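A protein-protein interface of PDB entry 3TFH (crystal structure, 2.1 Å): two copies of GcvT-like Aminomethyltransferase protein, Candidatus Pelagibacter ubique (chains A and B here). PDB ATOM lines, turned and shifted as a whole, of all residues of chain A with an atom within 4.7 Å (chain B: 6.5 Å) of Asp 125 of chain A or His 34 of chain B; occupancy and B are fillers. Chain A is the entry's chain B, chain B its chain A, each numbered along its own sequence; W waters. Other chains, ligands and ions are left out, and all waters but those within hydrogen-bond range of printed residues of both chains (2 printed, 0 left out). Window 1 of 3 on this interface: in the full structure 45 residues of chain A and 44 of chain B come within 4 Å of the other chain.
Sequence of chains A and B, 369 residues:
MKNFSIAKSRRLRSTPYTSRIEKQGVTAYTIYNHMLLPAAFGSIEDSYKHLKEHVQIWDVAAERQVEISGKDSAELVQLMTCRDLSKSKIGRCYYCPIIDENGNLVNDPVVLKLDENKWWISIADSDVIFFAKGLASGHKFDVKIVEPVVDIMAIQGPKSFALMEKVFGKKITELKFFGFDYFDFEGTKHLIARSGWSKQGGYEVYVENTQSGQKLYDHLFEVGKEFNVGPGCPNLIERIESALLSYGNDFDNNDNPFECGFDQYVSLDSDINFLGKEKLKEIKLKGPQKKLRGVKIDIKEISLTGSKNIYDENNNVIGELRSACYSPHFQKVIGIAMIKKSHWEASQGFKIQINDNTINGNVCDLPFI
NH2 of Arg 11 of chain B lies within salt-bridge range of OD1 of Asp 125 of chain A (2.9 Å). The backbone carbonyl oxygen of Ile 31 of chain A is in hydrogen-bond range of the guanidinium group of Arg 11 of chain B, at 2.8 Å. A ring nitrogen (ND1) of His 34 of chain B sits at hydrogen-bond distance from the side-chain carboxylate (OD1) of Asp 125 of chain A, 3.0 Å away.
The side-chain hydroxyl (OG) of Ser 126 of chain A sits at hydrogen-bond distance from the side-chain amide nitrogen (ND2) of Asn 107 of chain A, 2.7 Å away. The side-chain amide oxygen (OD1) of Asn 33 of chain A lies within hydrogen-bond range of the backbone NH (N) of Ser 126 of chain A, 3.3 Å away. OD1 of Asp 127 of chain B lies within hydrogen-bond range of NE2 of His 34 of chain B, at 2.7 Å. NE of Arg 13 of chain B sits at hydrogen-bond distance from O of His 34 of chain B, at 3.0 Å. The side-chain carboxylate (OD2) of Asp 125 of chain A lies within hydrogen-bond range of the backbone NH (N) of Asn 33 of chain A, at 2.8 Å.
CD2 of Leu 12 of chain B touches O of Ile 31 of chain A, 3.6 Å away. Ile 31 of chain B touches Ile 31 of chain A (CB to CB, 3.8 Å). CD1 of Tyr 32 of chain A touches CZ of Arg 11 of chain B, 3.7 Å away. Ser 126 of chain A touches Asp 127 of chain B (CA to OD2, 3.4 Å). CE2 of Phe 130 of chain B touches CB of Ser 126 of chain A, at 3.9 Å. Tyr 247 of chain A touches Arg 11 of chain B (O to CD, 3.3 Å). OH of Tyr 247 of chain A touches CZ of Phe 130 of chain B, 3.7 Å away.
His 34 of chain B touches one residue of chain A. Of the printed residues of chain B, Tyr 247 of chain A touches Arg 11 (3.3 Å) and Phe 130 (3.7 Å). Printed residues of chain A within 4 Å of Ile 31 of chain B: Ile 31 (3.8 Å). Tyr 32 of chain B touches none of the printed residues of chain A. Asp 125 of chain B touches none of the printed residues of chain A. The nearest residue of chain B that does not touch Asp 125 of chain A is Asp 127 of chain B (4.9 Å). The nearest residue of chain A that does not touch His 34 of chain B is Ser 126 of chain A (4.3 Å). The nearest printed residue of chain A that does not touch Asp 127 of chain B is Asp 125 of chain A (4.9 Å).
Printed residues of chain A that touch a printed residue of chain B: Ile 31, Tyr 32, Asp 125, Ser 126 and Tyr 247. Hydrophobic or aromatic side chains of chain A that line the printed part of chain B: Ile 31, Tyr 32 and Tyr 247. Of the 16 printed residues of chain B, 6 touch a printed residue of chain A. Among the printed residues, Asp or Glu carboxylates within 4 Å of a Lys or Arg side-chain nitrogen of the other chain: Asp 125 of chain A with Arg 11 of chain B.
Ile 31 of chain B touches its own counterpart, Ile 31 of chain A. Positions printed for both chains: 31, 32, 33, 125 and 126.
Water W1 lies within hydrogen-bond range of the backbone carbonyl oxygen (O) of Ile 31 of chain A (2.9 Å), the side-chain carboxylate (OD1) of Asp 125 of chain A (3.0 Å) and a ring nitrogen (ND1) of His 34 of chain B (3.2 Å). Water W2 lies within hydrogen-bond range of the side-chain carboxylate (OD2) of Asp 125 of chain A (3.0 Å), the backbone NH (N) of Asn 33 of chain A (3.3 Å) and a ring nitrogen (ND1) of His 34 of chain B (3.3 Å).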
ATOM      1  N   ILE A  31      -0.207   6.426  30.313  1.00  0.00           N
ATOM      2  CA  ILE A  31      -0.304   6.152  28.908  1.00  0.00           C
ATOM      3  C   ILE A  31       1.113   5.793  28.423  1.00  0.00           C
ATOM      4  O   ILE A  31       2.107   6.457  28.727  1.00  0.00           O
ATOM      5  CB  ILE A  31      -0.938   7.317  28.094  1.00  0.00           C
ATOM      6  CG1 ILE A  31      -2.429   7.453  28.469  1.00  0.00           C
ATOM      7  CG2 ILE A  31      -0.693   7.152  26.547  1.00  0.00           C
ATOM      8  CD1 ILE A  31      -3.322   6.228  28.070  1.00  0.00           C
ATOM      9  N   TYR A  32       1.163   4.702  27.686  1.00  0.00           N
ATOM     10  CA  TYR A  32       2.414   4.078  27.260  1.00  0.00           C
ATOM     11  C   TYR A  32       2.144   3.509  25.878  1.00  0.00           C
ATOM     12  O   TYR A  32       1.181   2.735  25.703  1.00  0.00           O
ATOM     13  CB  TYR A  32       2.737   2.999  28.254  1.00  0.00           C
ATOM     14  CG  TYR A  32       4.184   2.539  28.332  1.00  0.00           C
ATOM     15  CD1 TYR A  32       4.994   2.925  29.367  1.00  0.00           C
ATOM     16  CD2 TYR A  32       4.685   1.643  27.415  1.00  0.00           C
ATOM     17  CE1 TYR A  32       6.332   2.466  29.456  1.00  0.00           C
ATOM     18  CE2 TYR A  32       6.025   1.194  27.472  1.00  0.00           C
ATOM     19  CZ  TYR A  32       6.842   1.612  28.471  1.00  0.00           C
ATOM     20  OH  TYR A  32       8.132   1.061  28.546  1.00  0.00           O
ATOM     21  N   ASN A  33       2.911   3.965  24.868  1.00  0.00           N
ATOM     22  CA  ASN A  33       2.633   3.566  23.497  1.00  0.00           C
ATOM     23  C   ASN A  33       1.123   3.738  23.107  1.00  0.00           C
ATOM     24  O   ASN A  33       0.472   2.846  22.522  1.00  0.00           O
ATOM     25  CB  ASN A  33       3.081   2.130  23.299  1.00  0.00           C
ATOM     26  CG  ASN A  33       4.596   2.010  23.221  1.00  0.00           C
ATOM     27  OD1 ASN A  33       5.278   2.865  22.624  1.00  0.00           O
ATOM     28  ND2 ASN A  33       5.134   0.980  23.832  1.00  0.00           N
ATOM     29  N   ASN A 107      14.747   4.109  22.093  1.00  0.00           N
ATOM     30  CA  ASN A 107      13.950   3.123  22.810  1.00  0.00           C
ATOM     31  C   ASN A 107      14.934   2.093  23.379  1.00  0.00           C
ATOM     32  O   ASN A 107      16.031   1.875  22.794  1.00  0.00           O
ATOM     33  CB  ASN A 107      13.025   2.430  21.808  1.00  0.00           C
ATOM     34  CG  ASN A 107      11.819   1.771  22.478  1.00  0.00           C
ATOM     35  OD1 ASN A 107      11.876   0.628  22.971  1.00  0.00           O
ATOM     36  ND2 ASN A 107      10.721   2.490  22.459  1.00  0.00           N
ATOM     37  N   ILE A 123       8.732  -3.133  23.001  1.00  0.00           N
ATOM     38  CA  ILE A 123       9.161  -1.731  23.106  1.00  0.00           C
ATOM     39  C   ILE A 123       8.751  -0.959  24.327  1.00  0.00           C
ATOM     40  O   ILE A 123       7.700  -1.207  24.951  1.00  0.00           O
ATOM     41  CB  ILE A 123       8.757  -0.964  21.852  1.00  0.00           C
ATOM     42  CG1 ILE A 123       7.248  -1.027  21.641  1.00  0.00           C
ATOM     43  CG2 ILE A 123       9.552  -1.521  20.613  1.00  0.00           C
ATOM     44  CD1 ILE A 123       6.674   0.111  20.903  1.00  0.00           C
ATOM     45  N   ALA A 124       9.678  -0.076  24.725  1.00  0.00           N
ATOM     46  CA  ALA A 124       9.448   1.040  25.597  1.00  0.00           C
ATOM     47  C   ALA A 124       8.522   2.097  24.918  1.00  0.00           C
ATOM     48  O   ALA A 124       7.986   1.903  23.821  1.00  0.00           O
ATOM     49  CB  ALA A 124      10.830   1.670  26.024  1.00  0.00           C
ATOM     50  N   ASP A 125       8.373   3.243  25.563  1.00  0.00           N
ATOM     51  CA  ASP A 125       7.371   4.223  25.142  1.00  0.00           C
ATOM     52  C   ASP A 125       7.876   5.155  24.045  1.00  0.00           C
ATOM     53  O   ASP A 125       8.110   6.326  24.268  1.00  0.00           O
ATOM     54  CB  ASP A 125       6.887   4.985  26.376  1.00  0.00           C
ATOM     55  CG  ASP A 125       5.836   6.028  26.055  1.00  0.00           C
ATOM     56  OD1 ASP A 125       5.844   7.094  26.737  1.00  0.00           O
ATOM     57  OD2 ASP A 125       4.999   5.797  25.143  1.00  0.00           O
ATOM     58  N   SER A 126       8.017   4.623  22.838  1.00  0.00           N
ATOM     59  CA  SER A 126       8.215   5.459  21.648  1.00  0.00           C
ATOM     60  C   SER A 126       7.868   4.635  20.444  1.00  0.00           C
ATOM     61  O   SER A 126       7.932   3.404  20.523  1.00  0.00           O
ATOM     62  CB  SER A 126       9.663   5.965  21.513  1.00  0.00           C
ATOM     63  OG  SER A 126      10.506   4.869  21.248  1.00  0.00           O
ATOM     64  N   TYR A 247      12.859   4.590  29.563  1.00  0.00           N
ATOM     65  CA  TYR A 247      12.930   5.550  28.501  1.00  0.00           C
ATOM     66  C   TYR A 247      11.854   6.631  28.674  1.00  0.00           C
ATOM     67  O   TYR A 247      10.711   6.312  28.959  1.00  0.00           O
ATOM     68  CB  TYR A 247      12.780   4.908  27.123  1.00  0.00           C
ATOM     69  CG  TYR A 247      12.774   5.931  26.009  1.00  0.00           C
ATOM     70  CD1 TYR A 247      13.960   6.456  25.506  1.00  0.00           C
ATOM     71  CD2 TYR A 247      11.572   6.425  25.488  1.00  0.00           C
ATOM     72  CE1 TYR A 247      13.945   7.425  24.483  1.00  0.00           C
ATOM     73  CE2 TYR A 247      11.559   7.398  24.510  1.00  0.00           C
ATOM     74  CZ  TYR A 247      12.754   7.871  24.002  1.00  0.00           C
ATOM     75  OH  TYR A 247      12.746   8.850  23.025  1.00  0.00           O
ATOM     76  N   ARG B  10       8.102  12.173  34.931  1.00  0.00           N
ATOM     77  CA  ARG B  10       8.910  12.861  33.940  1.00  0.00           C
ATOM     78  C   ARG B  10       8.524  12.421  32.496  1.00  0.00           C
ATOM     79  O   ARG B  10       8.501  13.265  31.570  1.00  0.00           O
ATOM     80  CB  ARG B  10      10.432  12.695  34.182  1.00  0.00           C
ATOM     81  CG  ARG B  10      11.321  13.518  33.300  1.00  0.00           C
ATOM     82  CD  ARG B  10      12.840  13.397  33.635  1.00  0.00           C
ATOM     83  NE  ARG B  10      13.583  14.232  32.693  1.00  0.00           N
ATOM     84  CZ  ARG B  10      13.970  13.916  31.468  1.00  0.00           C
ATOM     85  NH1 ARG B  10      13.807  12.701  30.947  1.00  0.00           N
ATOM     86  NH2 ARG B  10      14.570  14.834  30.743  1.00  0.00           N
ATOM     87  N   ARG B  11       8.238  11.138  32.296  1.00  0.00           N
ATOM     88  CA  ARG B  11       7.897  10.643  30.953  1.00  0.00           C
ATOM     89  C   ARG B  11       6.574  11.194  30.413  1.00  0.00           C
ATOM     90  O   ARG B  11       6.415  11.389  29.218  1.00  0.00           O
ATOM     91  CB  ARG B  11       7.883   9.126  30.921  1.00  0.00           C
ATOM     92  CG  ARG B  11       7.584   8.513  29.594  1.00  0.00           C
ATOM     93  CD  ARG B  11       7.615   7.014  29.677  1.00  0.00           C
ATOM     94  NE  ARG B  11       6.692   6.520  30.685  1.00  0.00           N
ATOM     95  CZ  ARG B  11       5.366   6.420  30.534  1.00  0.00           C
ATOM     96  NH1 ARG B  11       4.607   5.980  31.537  1.00  0.00           N
ATOM     97  NH2 ARG B  11       4.785   6.808  29.440  1.00  0.00           N
ATOM     98  N   LEU B  12       5.615  11.405  31.286  1.00  0.00           N
ATOM     99  CA  LEU B  12       4.345  12.015  30.878  1.00  0.00           C
ATOM    100  C   LEU B  12       4.489  13.471  31.153  1.00  0.00           C
ATOM    101  O   LEU B  12       4.122  13.948  32.240  1.00  0.00           O
ATOM    102  CB  LEU B  12       3.164  11.484  31.654  1.00  0.00           C
ATOM    103  CG  LEU B  12       2.673  10.092  31.361  1.00  0.00           C
ATOM    104  CD1 LEU B  12       1.258  10.032  31.949  1.00  0.00           C
ATOM    105  CD2 LEU B  12       2.655   9.822  29.897  1.00  0.00           C
ATOM    106  N   ARG B  13       5.065  14.174  30.167  1.00  0.00           N
ATOM    107  CA  ARG B  13       5.596  15.542  30.297  1.00  0.00           C
ATOM    108  C   ARG B  13       4.555  16.648  30.644  1.00  0.00           C
ATOM    109  O   ARG B  13       3.487  16.688  30.099  1.00  0.00           O
ATOM    110  CB  ARG B  13       6.367  15.938  29.010  1.00  0.00           C
ATOM    111  CG  ARG B  13       7.563  15.035  28.688  1.00  0.00           C
ATOM    112  CD  ARG B  13       8.208  15.406  27.360  1.00  0.00           C
ATOM    113  NE  ARG B  13       7.381  15.031  26.199  1.00  0.00           N
ATOM    114  CZ  ARG B  13       7.690  15.355  24.937  1.00  0.00           C
ATOM    115  NH1 ARG B  13       8.804  16.038  24.695  1.00  0.00           N
ATOM    116  NH2 ARG B  13       6.897  15.027  23.904  1.00  0.00           N
ATOM    117  N   SER B  14       4.941  17.511  31.595  1.00  0.00           N
ATOM    118  CA  SER B  14       4.129  18.670  31.889  1.00  0.00           C
ATOM    119  C   SER B  14       4.614  19.736  30.895  1.00  0.00           C
ATOM    120  O   SER B  14       5.510  19.487  30.058  1.00  0.00           O
ATOM    121  CB  SER B  14       4.237  19.045  33.383  1.00  0.00           C
ATOM    122  OG  SER B  14       3.728  17.992  34.233  1.00  0.00           O
ATOM    123  N   ILE B  31      -3.399  12.415  27.157  1.00  0.00           N
ATOM    124  CA  ILE B  31      -2.007  12.348  26.886  1.00  0.00           C
ATOM    125  C   ILE B  31      -1.918  12.396  25.340  1.00  0.00           C
ATOM    126  O   ILE B  31      -2.632  11.677  24.642  1.00  0.00           O
ATOM    127  CB  ILE B  31      -1.273  11.096  27.442  1.00  0.00           C
ATOM    128  CG1 ILE B  31      -1.079  11.118  28.986  1.00  0.00           C
ATOM    129  CG2 ILE B  31       0.210  10.916  26.746  1.00  0.00           C
ATOM    130  CD1 ILE B  31      -0.534  12.359  29.569  1.00  0.00           C
ATOM    131  N   TYR B  32      -1.014  13.228  24.850  1.00  0.00           N
ATOM    132  CA  TYR B  32      -0.802  13.433  23.417  1.00  0.00           C
ATOM    133  C   TYR B  32       0.707  13.610  23.249  1.00  0.00           C
ATOM    134  O   TYR B  32       1.305  14.485  23.898  1.00  0.00           O
ATOM    135  CB  TYR B  32      -1.571  14.687  23.076  1.00  0.00           C
ATOM    136  CG  TYR B  32      -1.992  14.904  21.695  1.00  0.00           C
ATOM    137  CD1 TYR B  32      -3.244  14.548  21.257  1.00  0.00           C
ATOM    138  CD2 TYR B  32      -1.143  15.576  20.816  1.00  0.00           C
ATOM    139  CE1 TYR B  32      -3.655  14.821  19.942  1.00  0.00           C
ATOM    140  CE2 TYR B  32      -1.536  15.876  19.509  1.00  0.00           C
ATOM    141  CZ  TYR B  32      -2.777  15.491  19.080  1.00  0.00           C
ATOM    142  OH  TYR B  32      -3.091  15.811  17.786  1.00  0.00           O
ATOM    143  N   ASN B  33       1.340  12.799  22.403  1.00  0.00           N
ATOM    144  CA  ASN B  33       2.791  12.888  22.233  1.00  0.00           C
ATOM    145  C   ASN B  33       3.568  12.870  23.547  1.00  0.00           C
ATOM    146  O   ASN B  33       4.439  13.735  23.769  1.00  0.00           O
ATOM    147  CB  ASN B  33       3.136  14.151  21.420  1.00  0.00           C
ATOM    148  CG  ASN B  33       2.690  14.055  19.966  1.00  0.00           C
ATOM    149  OD1 ASN B  33       2.995  13.063  19.289  1.00  0.00           O
ATOM    150  ND2 ASN B  33       2.004  15.080  19.474  1.00  0.00           N
ATOM    151  N   HIS B  34       3.222  11.937  24.460  1.00  0.00           N
ATOM    152  CA  HIS B  34       3.956  11.755  25.685  1.00  0.00           C
ATOM    153  C   HIS B  34       3.977  13.073  26.484  1.00  0.00           C
ATOM    154  O   HIS B  34       4.990  13.390  27.122  1.00  0.00           O
ATOM    155  CB  HIS B  34       5.437  11.289  25.406  1.00  0.00           C
ATOM    156  CG  HIS B  34       5.587  10.324  24.275  1.00  0.00           C
ATOM    157  ND1 HIS B  34       5.298   8.974  24.399  1.00  0.00           N
ATOM    158  CD2 HIS B  34       5.991  10.507  23.000  1.00  0.00           C
ATOM    159  CE1 HIS B  34       5.562   8.376  23.256  1.00  0.00           C
ATOM    160  NE2 HIS B  34       5.957   9.280  22.389  1.00  0.00           N
ATOM    161  N   MET B  35       2.847  13.795  26.461  1.00  0.00           N
ATOM    162  CA  MET B  35       2.730  15.068  27.111  1.00  0.00           C
ATOM    163  C   MET B  35       1.279  15.281  27.555  1.00  0.00           C
ATOM    164  O   MET B  35       0.319  14.845  26.901  1.00  0.00           O
ATOM    165  CB  MET B  35       3.163  16.230  26.162  1.00  0.00           C
ATOM    166  CG  MET B  35       3.279  17.556  26.856  1.00  0.00           C
ATOM    167  SD  MET B  35       4.042  18.820  25.845  1.00  0.00           S
ATOM    168  CE  MET B  35       5.778  18.495  26.226  1.00  0.00           C
ATOM    169  N   LEU B  36       1.139  15.942  28.682  1.00  0.00           N
ATOM    170  CA  LEU B  36      -0.195  16.286  29.186  1.00  0.00           C
ATOM    171  C   LEU B  36      -0.867  17.332  28.297  1.00  0.00           C
ATOM    172  O   LEU B  36      -0.259  18.351  27.928  1.00  0.00           O
ATOM    173  CB  LEU B  36      -0.119  16.803  30.616  1.00  0.00           C
ATOM    174  CG  LEU B  36       0.343  15.822  31.690  1.00  0.00           C
ATOM    175  CD1 LEU B  36       0.801  16.530  33.015  1.00  0.00           C
ATOM    176  CD2 LEU B  36      -0.780  14.840  31.964  1.00  0.00           C
ATOM    177  N   ALA B  62       1.395  20.025  23.710  1.00  0.00           N
ATOM    178  CA  ALA B  62       1.533  18.610  23.264  1.00  0.00           C
ATOM    179  C   ALA B  62       1.472  18.441  21.735  1.00  0.00           C
ATOM    180  O   ALA B  62       1.753  17.367  21.196  1.00  0.00           O
ATOM    181  CB  ALA B  62       0.449  17.708  23.954  1.00  0.00           C
ATOM    182  N   ASP B 125      -0.818  12.922  17.159  1.00  0.00           N
ATOM    183  CA  ASP B 125      -0.294  12.023  18.211  1.00  0.00           C
ATOM    184  C   ASP B 125       0.390  10.782  17.661  1.00  0.00           C
ATOM    185  O   ASP B 125      -0.168   9.664  17.707  1.00  0.00           O
ATOM    186  CB  ASP B 125      -1.444  11.604  19.133  1.00  0.00           C
ATOM    187  CG  ASP B 125      -1.006  10.729  20.317  1.00  0.00           C
ATOM    188  OD1 ASP B 125      -1.849   9.915  20.739  1.00  0.00           O
ATOM    189  OD2 ASP B 125       0.116  10.866  20.829  1.00  0.00           O
ATOM    190  N   SER B 126       1.650  10.965  17.252  1.00  0.00           N
ATOM    191  CA  SER B 126       2.548   9.863  16.923  1.00  0.00           C
ATOM    192  C   SER B 126       3.956  10.445  16.732  1.00  0.00           C
ATOM    193  O   SER B 126       4.088  11.643  16.465  1.00  0.00           O
ATOM    194  CB  SER B 126       2.103   9.079  15.659  1.00  0.00           C
ATOM    195  OG  SER B 126       2.312   9.777  14.466  1.00  0.00           O
ATOM    196  N   ASP B 127       4.979   9.598  16.867  1.00  0.00           N
ATOM    197  CA  ASP B 127       6.367  10.050  16.904  1.00  0.00           C
ATOM    198  C   ASP B 127       6.997  10.206  15.494  1.00  0.00           C
ATOM    199  O   ASP B 127       7.920   9.444  15.063  1.00  0.00           O
ATOM    200  CB  ASP B 127       7.210   9.190  17.784  1.00  0.00           C
ATOM    201  CG  ASP B 127       6.724   9.149  19.240  1.00  0.00           C
ATOM    202  OD1 ASP B 127       6.148  10.136  19.792  1.00  0.00           O
ATOM    203  OD2 ASP B 127       7.059   8.161  19.876  1.00  0.00           O
ATOM    204  N   PHE B 130      10.649  10.110  14.695  1.00  0.00           N
ATOM    205  CA  PHE B 130      11.411   8.895  14.460  1.00  0.00           C
ATOM    206  C   PHE B 130      11.178   8.360  13.038  1.00  0.00           C
ATOM    207  O   PHE B 130      12.032   7.692  12.475  1.00  0.00           O
ATOM    208  CB  PHE B 130      11.222   7.844  15.578  1.00  0.00           C
ATOM    209  CG  PHE B 130      11.729   8.281  16.890  1.00  0.00           C
ATOM    210  CD1 PHE B 130      13.039   8.757  17.034  1.00  0.00           C
ATOM    211  CD2 PHE B 130      10.915   8.236  18.015  1.00  0.00           C
ATOM    212  CE1 PHE B 130      13.517   9.162  18.229  1.00  0.00           C
ATOM    213  CE2 PHE B 130      11.366   8.669  19.224  1.00  0.00           C
ATOM    214  CZ  PHE B 130      12.674   9.128  19.363  1.00  0.00           C
HETATM  215  O   HOH W   1       3.057   8.280  26.636  1.00  0.00           O
HETATM  216  O   HOH W   2       2.629   7.081  23.793  1.00  0.00           O
